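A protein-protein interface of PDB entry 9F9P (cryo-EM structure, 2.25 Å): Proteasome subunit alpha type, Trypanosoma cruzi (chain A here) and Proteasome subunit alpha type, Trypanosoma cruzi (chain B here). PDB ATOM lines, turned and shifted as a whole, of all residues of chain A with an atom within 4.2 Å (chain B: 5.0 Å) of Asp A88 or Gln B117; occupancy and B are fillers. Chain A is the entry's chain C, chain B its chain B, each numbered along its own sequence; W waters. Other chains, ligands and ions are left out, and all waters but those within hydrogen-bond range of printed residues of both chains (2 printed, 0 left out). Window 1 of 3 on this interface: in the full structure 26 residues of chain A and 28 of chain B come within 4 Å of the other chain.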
ATOM      1  N   VAL A  85      11.853  19.484 -11.650  1.00  0.00           N
ATOM      2  CA  VAL A  85      11.735  20.912 -11.402  1.00  0.00           C
ATOM      3  C   VAL A  85      11.977  21.687 -12.709  1.00  0.00           C
ATOM      4  O   VAL A  85      13.066  21.720 -13.280  1.00  0.00           O
ATOM      5  CB  VAL A  85      12.702  21.290 -10.252  1.00  0.00           C
ATOM      6  CG1 VAL A  85      12.688  22.792  -9.920  1.00  0.00           C
ATOM      7  CG2 VAL A  85      12.465  20.450  -8.998  1.00  0.00           C
ATOM      8  N   THR A  86      10.950  22.371 -13.176  1.00  0.00           N
ATOM      9  CA  THR A  86      10.961  23.002 -14.483  1.00  0.00           C
ATOM     10  C   THR A  86      11.994  24.129 -14.611  1.00  0.00           C
ATOM     11  O   THR A  86      12.639  24.277 -15.651  1.00  0.00           O
ATOM     12  CB  THR A  86       9.576  23.566 -14.807  1.00  0.00           C
ATOM     13  OG1 THR A  86       8.630  22.494 -14.718  1.00  0.00           O
ATOM     14  CG2 THR A  86       9.537  24.182 -16.187  1.00  0.00           C
ATOM     15  N   SER A  87      12.158  24.964 -13.587  1.00  0.00           N
ATOM     16  CA  SER A  87      13.100  26.048 -13.793  1.00  0.00           C
ATOM     17  C   SER A  87      14.538  25.542 -13.756  1.00  0.00           C
ATOM     18  O   SER A  87      15.388  26.160 -14.399  1.00  0.00           O
ATOM     19  CB  SER A  87      12.848  27.215 -12.855  1.00  0.00           C
ATOM     20  OG  SER A  87      12.205  26.757 -11.669  1.00  0.00           O
ATOM     21  N   ASP A  88      14.787  24.425 -13.049  1.00  0.00           N
ATOM     22  CA  ASP A  88      16.099  23.775 -13.044  1.00  0.00           C
ATOM     23  C   ASP A  88      16.402  23.198 -14.421  1.00  0.00           C
ATOM     24  O   ASP A  88      17.534  23.252 -14.865  1.00  0.00           O
ATOM     25  CB  ASP A  88      16.206  22.647 -12.004  1.00  0.00           C
ATOM     26  CG  ASP A  88      16.384  23.041 -10.512  1.00  0.00           C
ATOM     27  OD1 ASP A  88      16.343  24.263 -10.163  1.00  0.00           O
ATOM     28  OD2 ASP A  88      16.552  22.097  -9.660  1.00  0.00           O
ATOM     29  N   ALA A  89      15.389  22.634 -15.089  1.00  0.00           N
ATOM     30  CA  ALA A  89      15.571  22.123 -16.430  1.00  0.00           C
ATOM     31  C   ALA A  89      16.007  23.215 -17.387  1.00  0.00           C
ATOM     32  O   ALA A  89      16.926  22.976 -18.135  1.00  0.00           O
ATOM     33  CB  ALA A  89      14.322  21.479 -16.921  1.00  0.00           C
ATOM     34  N   TYR A  90      15.386  24.387 -17.356  1.00  0.00           N
ATOM     35  CA  TYR A  90      15.817  25.502 -18.179  1.00  0.00           C
ATOM     36  C   TYR A  90      17.269  25.891 -17.927  1.00  0.00           C
ATOM     37  O   TYR A  90      17.973  26.189 -18.874  1.00  0.00           O
ATOM     38  CB  TYR A  90      14.929  26.747 -18.028  1.00  0.00           C
ATOM     39  CG  TYR A  90      13.688  26.726 -18.879  1.00  0.00           C
ATOM     40  CD1 TYR A  90      13.721  27.144 -20.205  1.00  0.00           C
ATOM     41  CD2 TYR A  90      12.486  26.257 -18.387  1.00  0.00           C
ATOM     42  CE1 TYR A  90      12.583  27.115 -21.007  1.00  0.00           C
ATOM     43  CE2 TYR A  90      11.342  26.195 -19.172  1.00  0.00           C
ATOM     44  CZ  TYR A  90      11.386  26.630 -20.489  1.00  0.00           C
ATOM     45  OH  TYR A  90      10.241  26.583 -21.263  1.00  0.00           O
ATOM     46  N   ALA A  91      17.757  25.890 -16.701  1.00  0.00           N
ATOM     47  CA  ALA A  91      19.161  26.190 -16.485  1.00  0.00           C
ATOM     48  C   ALA A  91      20.082  25.162 -17.130  1.00  0.00           C
ATOM     49  O   ALA A  91      21.080  25.541 -17.736  1.00  0.00           O
ATOM     50  CB  ALA A  91      19.452  26.303 -15.026  1.00  0.00           C
ATOM     51  N   LEU A  92      19.767  23.868 -17.051  1.00  0.00           N
ATOM     52  CA  LEU A  92      20.631  22.875 -17.675  1.00  0.00           C
ATOM     53  C   LEU A  92      20.473  22.850 -19.189  1.00  0.00           C
ATOM     54  O   LEU A  92      21.420  22.537 -19.890  1.00  0.00           O
ATOM     55  CB  LEU A  92      20.326  21.492 -17.099  1.00  0.00           C
ATOM     56  CG  LEU A  92      20.850  21.255 -15.681  1.00  0.00           C
ATOM     57  CD1 LEU A  92      20.419  19.905 -15.153  1.00  0.00           C
ATOM     58  CD2 LEU A  92      22.332  21.307 -15.649  1.00  0.00           C
ATOM     59  N   ARG A 134      21.903  22.828  -2.845  1.00  0.00           N
ATOM     60  CA  ARG A 134      21.119  21.665  -3.246  1.00  0.00           C
ATOM     61  C   ARG A 134      21.488  21.251  -4.667  1.00  0.00           C
ATOM     62  O   ARG A 134      21.914  22.070  -5.471  1.00  0.00           O
ATOM     63  CB  ARG A 134      19.613  21.930  -3.188  1.00  0.00           C
ATOM     64  CG  ARG A 134      19.118  22.961  -4.196  1.00  0.00           C
ATOM     65  CD  ARG A 134      17.619  22.988  -4.248  1.00  0.00           C
ATOM     66  NE  ARG A 134      17.063  23.973  -5.183  1.00  0.00           N
ATOM     67  CZ  ARG A 134      16.851  23.748  -6.474  1.00  0.00           C
ATOM     68  NH1 ARG A 134      17.096  22.564  -7.003  1.00  0.00           N
ATOM     69  NH2 ARG A 134      16.404  24.719  -7.240  1.00  0.00           N
ATOM     70  N   PHE A 136      20.550  19.741  -8.653  1.00  0.00           N
ATOM     71  CA  PHE A 136      19.455  19.902  -9.617  1.00  0.00           C
ATOM     72  C   PHE A 136      18.439  18.786  -9.434  1.00  0.00           C
ATOM     73  O   PHE A 136      18.808  17.660  -9.137  1.00  0.00           O
ATOM     74  CB  PHE A 136      19.997  19.897 -11.050  1.00  0.00           C
ATOM     75  CG  PHE A 136      20.793  21.121 -11.410  1.00  0.00           C
ATOM     76  CD1 PHE A 136      20.165  22.333 -11.652  1.00  0.00           C
ATOM     77  CD2 PHE A 136      22.170  21.082 -11.441  1.00  0.00           C
ATOM     78  CE1 PHE A 136      20.898  23.461 -11.974  1.00  0.00           C
ATOM     79  CE2 PHE A 136      22.904  22.211 -11.757  1.00  0.00           C
ATOM     80  CZ  PHE A 136      22.264  23.398 -12.021  1.00  0.00           C
ATOM     81  N   GLY A 137      17.156  19.089  -9.605  1.00  0.00           N
ATOM     82  CA  GLY A 137      16.124  18.060  -9.486  1.00  0.00           C
ATOM     83  C   GLY A 137      15.493  17.747 -10.828  1.00  0.00           C
ATOM     84  O   GLY A 137      14.295  17.896 -10.971  1.00  0.00           O
ATOM     85  N   VAL A 138      16.299  17.217 -11.766  1.00  0.00           N
ATOM     86  CA  VAL A 138      15.873  16.980 -13.141  1.00  0.00           C
ATOM     87  C   VAL A 138      16.324  15.614 -13.645  1.00  0.00           C
ATOM     88  O   VAL A 138      17.430  15.201 -13.358  1.00  0.00           O
ATOM     89  CB  VAL A 138      16.468  18.078 -14.035  1.00  0.00           C
ATOM     90  CG1 VAL A 138      16.109  17.866 -15.475  1.00  0.00           C
ATOM     91  CG2 VAL A 138      15.965  19.432 -13.651  1.00  0.00           C
ATOM     92  N   SER B 113      12.544  34.918 -15.120  1.00  0.00           N
ATOM     93  CA  SER B 113      12.434  33.557 -14.615  1.00  0.00           C
ATOM     94  C   SER B 113      13.766  32.980 -14.186  1.00  0.00           C
ATOM     95  O   SER B 113      13.845  32.226 -13.223  1.00  0.00           O
ATOM     96  CB  SER B 113      11.854  32.697 -15.674  1.00  0.00           C
ATOM     97  OG  SER B 113      11.788  31.367 -15.250  1.00  0.00           O
ATOM     98  N   SER B 114      14.836  33.283 -14.896  1.00  0.00           N
ATOM     99  CA  SER B 114      16.128  32.749 -14.498  1.00  0.00           C
ATOM    100  C   SER B 114      16.698  33.467 -13.284  1.00  0.00           C
ATOM    101  O   SER B 114      17.439  32.855 -12.550  1.00  0.00           O
ATOM    102  CB  SER B 114      17.101  32.764 -15.641  1.00  0.00           C
ATOM    103  OG  SER B 114      17.606  34.059 -15.766  1.00  0.00           O
ATOM    104  N   LEU B 115      16.363  34.734 -13.060  1.00  0.00           N
ATOM    105  CA  LEU B 115      16.688  35.421 -11.809  1.00  0.00           C
ATOM    106  C   LEU B 115      15.933  34.857 -10.600  1.00  0.00           C
ATOM    107  O   LEU B 115      16.572  34.581  -9.609  1.00  0.00           O
ATOM    108  CB  LEU B 115      16.474  36.929 -11.997  1.00  0.00           C
ATOM    109  CG  LEU B 115      16.689  37.773 -10.743  1.00  0.00           C
ATOM    110  CD1 LEU B 115      18.127  37.691 -10.216  1.00  0.00           C
ATOM    111  CD2 LEU B 115      16.325  39.256 -10.988  1.00  0.00           C
ATOM    112  N   TYR B 116      14.637  34.544 -10.700  1.00  0.00           N
ATOM    113  CA  TYR B 116      13.954  33.758  -9.681  1.00  0.00           C
ATOM    114  C   TYR B 116      14.637  32.401  -9.409  1.00  0.00           C
ATOM    115  O   TYR B 116      14.805  32.007  -8.273  1.00  0.00           O
ATOM    116  CB  TYR B 116      12.511  33.454 -10.073  1.00  0.00           C
ATOM    117  CG  TYR B 116      11.415  34.478  -9.840  1.00  0.00           C
ATOM    118  CD1 TYR B 116      10.819  34.603  -8.610  1.00  0.00           C
ATOM    119  CD2 TYR B 116      10.818  35.187 -10.867  1.00  0.00           C
ATOM    120  CE1 TYR B 116       9.739  35.440  -8.361  1.00  0.00           C
ATOM    121  CE2 TYR B 116       9.713  36.020 -10.646  1.00  0.00           C
ATOM    122  CZ  TYR B 116       9.145  36.133  -9.387  1.00  0.00           C
ATOM    123  OH  TYR B 116       8.105  36.951  -9.061  1.00  0.00           O
ATOM    124  N   GLN B 117      15.036  31.646 -10.430  1.00  0.00           N
ATOM    125  CA  GLN B 117      15.628  30.332 -10.236  1.00  0.00           C
ATOM    126  C   GLN B 117      16.931  30.388  -9.452  1.00  0.00           C
ATOM    127  O   GLN B 117      17.181  29.468  -8.704  1.00  0.00           O
ATOM    128  CB  GLN B 117      15.916  29.641 -11.580  1.00  0.00           C
ATOM    129  CG  GLN B 117      16.246  28.145 -11.522  1.00  0.00           C
ATOM    130  CD  GLN B 117      17.689  27.802 -11.211  1.00  0.00           C
ATOM    131  OE1 GLN B 117      18.644  28.532 -11.509  1.00  0.00           O
ATOM    132  NE2 GLN B 117      17.850  26.670 -10.537  1.00  0.00           N
ATOM    133  N   GLU B 118      17.764  31.414  -9.646  1.00  0.00           N
ATOM    134  CA  GLU B 118      18.998  31.558  -8.874  1.00  0.00           C
ATOM    135  C   GLU B 118      18.770  31.720  -7.372  1.00  0.00           C
ATOM    136  O   GLU B 118      19.555  31.221  -6.606  1.00  0.00           O
ATOM    137  CB  GLU B 118      19.813  32.788  -9.258  1.00  0.00           C
ATOM    138  CG  GLU B 118      20.546  32.670 -10.572  1.00  0.00           C
ATOM    139  CD  GLU B 118      21.073  34.018 -11.077  1.00  0.00           C
ATOM    140  OE1 GLU B 118      21.697  34.755 -10.260  1.00  0.00           O
ATOM    141  OE2 GLU B 118      20.840  34.352 -12.285  1.00  0.00           O
ATOM    142  N   PHE B 119      17.747  32.450  -6.942  1.00  0.00           N
ATOM    143  CA  PHE B 119      17.450  32.615  -5.522  1.00  0.00           C
ATOM    144  C   PHE B 119      16.792  31.364  -4.912  1.00  0.00           C
ATOM    145  O   PHE B 119      16.604  31.329  -3.699  1.00  0.00           O
ATOM    146  CB  PHE B 119      16.662  33.906  -5.275  1.00  0.00           C
ATOM    147  CG  PHE B 119      17.520  35.150  -5.343  1.00  0.00           C
ATOM    148  CD1 PHE B 119      17.891  35.839  -4.191  1.00  0.00           C
ATOM    149  CD2 PHE B 119      17.986  35.641  -6.565  1.00  0.00           C
ATOM    150  CE1 PHE B 119      18.746  36.939  -4.255  1.00  0.00           C
ATOM    151  CE2 PHE B 119      18.825  36.752  -6.632  1.00  0.00           C
ATOM    152  CZ  PHE B 119      19.203  37.406  -5.474  1.00  0.00           C
ATOM    153  N   THR B 120      16.570  30.293  -5.686  1.00  0.00           N
ATOM    154  CA  THR B 120      16.139  29.014  -5.126  1.00  0.00           C
ATOM    155  C   THR B 120      17.282  28.019  -4.975  1.00  0.00           C
ATOM    156  O   THR B 120      17.035  26.902  -4.566  1.00  0.00           O
ATOM    157  CB  THR B 120      15.115  28.260  -6.007  1.00  0.00           C
ATOM    158  OG1 THR B 120      15.638  27.802  -7.264  1.00  0.00           O
ATOM    159  CG2 THR B 120      13.901  29.102  -6.306  1.00  0.00           C
ATOM    160  N   GLN B 121      18.499  28.396  -5.342  1.00  0.00           N
ATOM    161  CA  GLN B 121      19.608  27.463  -5.348  1.00  0.00           C
ATOM    162  C   GLN B 121      20.913  28.047  -4.777  1.00  0.00           C
ATOM    163  O   GLN B 121      21.599  27.367  -4.026  1.00  0.00           O
ATOM    164  CB  GLN B 121      19.870  26.981  -6.768  1.00  0.00           C
ATOM    165  CG  GLN B 121      20.778  25.763  -6.809  1.00  0.00           C
ATOM    166  CD  GLN B 121      20.908  25.124  -8.166  1.00  0.00           C
ATOM    167  OE1 GLN B 121      20.679  25.753  -9.197  1.00  0.00           O
ATOM    168  NE2 GLN B 121      21.286  23.851  -8.177  1.00  0.00           N
ATOM    169  N   SER B 150       8.889  29.950  -7.879  1.00  0.00           N
ATOM    170  CA  SER B 150       9.679  28.852  -8.414  1.00  0.00           C
ATOM    171  C   SER B 150      10.440  29.243  -9.671  1.00  0.00           C
ATOM    172  O   SER B 150      11.424  28.618 -10.000  1.00  0.00           O
ATOM    173  CB  SER B 150       8.806  27.689  -8.697  1.00  0.00           C
ATOM    174  OG  SER B 150       7.764  28.023  -9.609  1.00  0.00           O
ATOM    175  N   GLY B 151       9.928  30.207 -10.420  1.00  0.00           N
ATOM    176  CA  GLY B 151      10.501  30.612 -11.687  1.00  0.00           C
ATOM    177  C   GLY B 151       9.677  30.086 -12.861  1.00  0.00           C
ATOM    178  O   GLY B 151       9.917  30.466 -14.020  1.00  0.00           O
HETATM  179  O   HOH W   1      20.422  25.609  -2.120  1.00  0.00           O
HETATM  180  O   HOH W   2      14.070  25.953  -9.688  1.00  0.00           O
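Water W2 lies within hydrogen-bond range of the side-chain hydroxyl of Ser A87 (2.8 Å), the side-chain carboxylate of Asp A88 (2.9 Å) and the side-chain hydroxyl of Thr B120 (3.4 Å).
Water W1 lies within hydrogen-bond range of O of Gln B121 and N of Arg A134.
The side-chain amide nitrogen (NE2) of Gln B117 lies within hydrogen-bond range of the side-chain carboxylate (OD1) of Asp A88 (2.9 Å).
NE of Arg A134 sits at hydrogen-bond distance from O of Thr B120 (3.0 Å).
The backbone carbonyl oxygen (O) of Arg A134 lies within hydrogen-bond range of the side-chain amide nitrogen (NE2) of Gln B121, at 3.3 Å.
The backbone carbonyl oxygen of Ser B150 lies within hydrogen-bond range of the side-chain hydroxyl of Ser A87 (2.6 Å).
The backbone carbonyl oxygen of Gln B117 is in hydrogen-bond range of the side-chain hydroxyl of Thr B120 (2.7 Å).
NE2 of Gln B117 sits at hydrogen-bond distance from OE1 of Gln B121, at 3.3 Å.
NH1 of Arg A134 lies within salt-bridge range of OD2 of Asp A88 (2.8 Å).
The side-chain carboxylate (OD2) of Asp A88 sits at hydrogen-bond distance from the backbone NH (N) of Gly A137 (3.1 Å).
Of the 12 printed residues of chain A, 4 touch a printed residue of chain B.
Hydrophobic or aromatic side chains of chain A within 4 Å of the printed part of chain B: Phe A136.
Printed residues of chain B that touch a printed residue of chain A: Gln B117, Thr B120, Gln B121 and Ser B150.
Of the printed residues of chain B, Ser A87 touches Gln B117 (3.6 Å) and Ser B150 (2.6 Å).
Asp A88 touches one residue of chain B.
Ala A91 touches none of the printed residues of chain B.
Printed residues of chain B within 4 Å of Arg A134: Thr B120 (3.0 Å) and Gln B121 (3.3 Å).
Of the printed residues of chain B, Phe A136 touches Gln B121 (3.6 Å).
Val A138 touches none of the printed residues of chain B.
Printed residues of chain A within 4 Å of Gln B117: Ser A87 and Asp A88.
Printed residues of chain A within 4 Å of Thr B120: Arg A134.
Of the printed residues of chain A, Gln B121 touches Arg A134 (3.3 Å) and Phe A136 (3.6 Å).
The nearest residue of chain B that does not touch Asp A88 is Thr B120 (4.6 Å).
The nearest residue of chain A that does not touch Gln B117 is Arg A134 (4.1 Å).
The nearest printed residue of chain A that does not touch Thr B120 is Asp A88 (4.6 Å).
Among the printed residues, pairs that only touch across the chains: Ser A87 with Gln B117 and Phe A136 with Gln B121.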
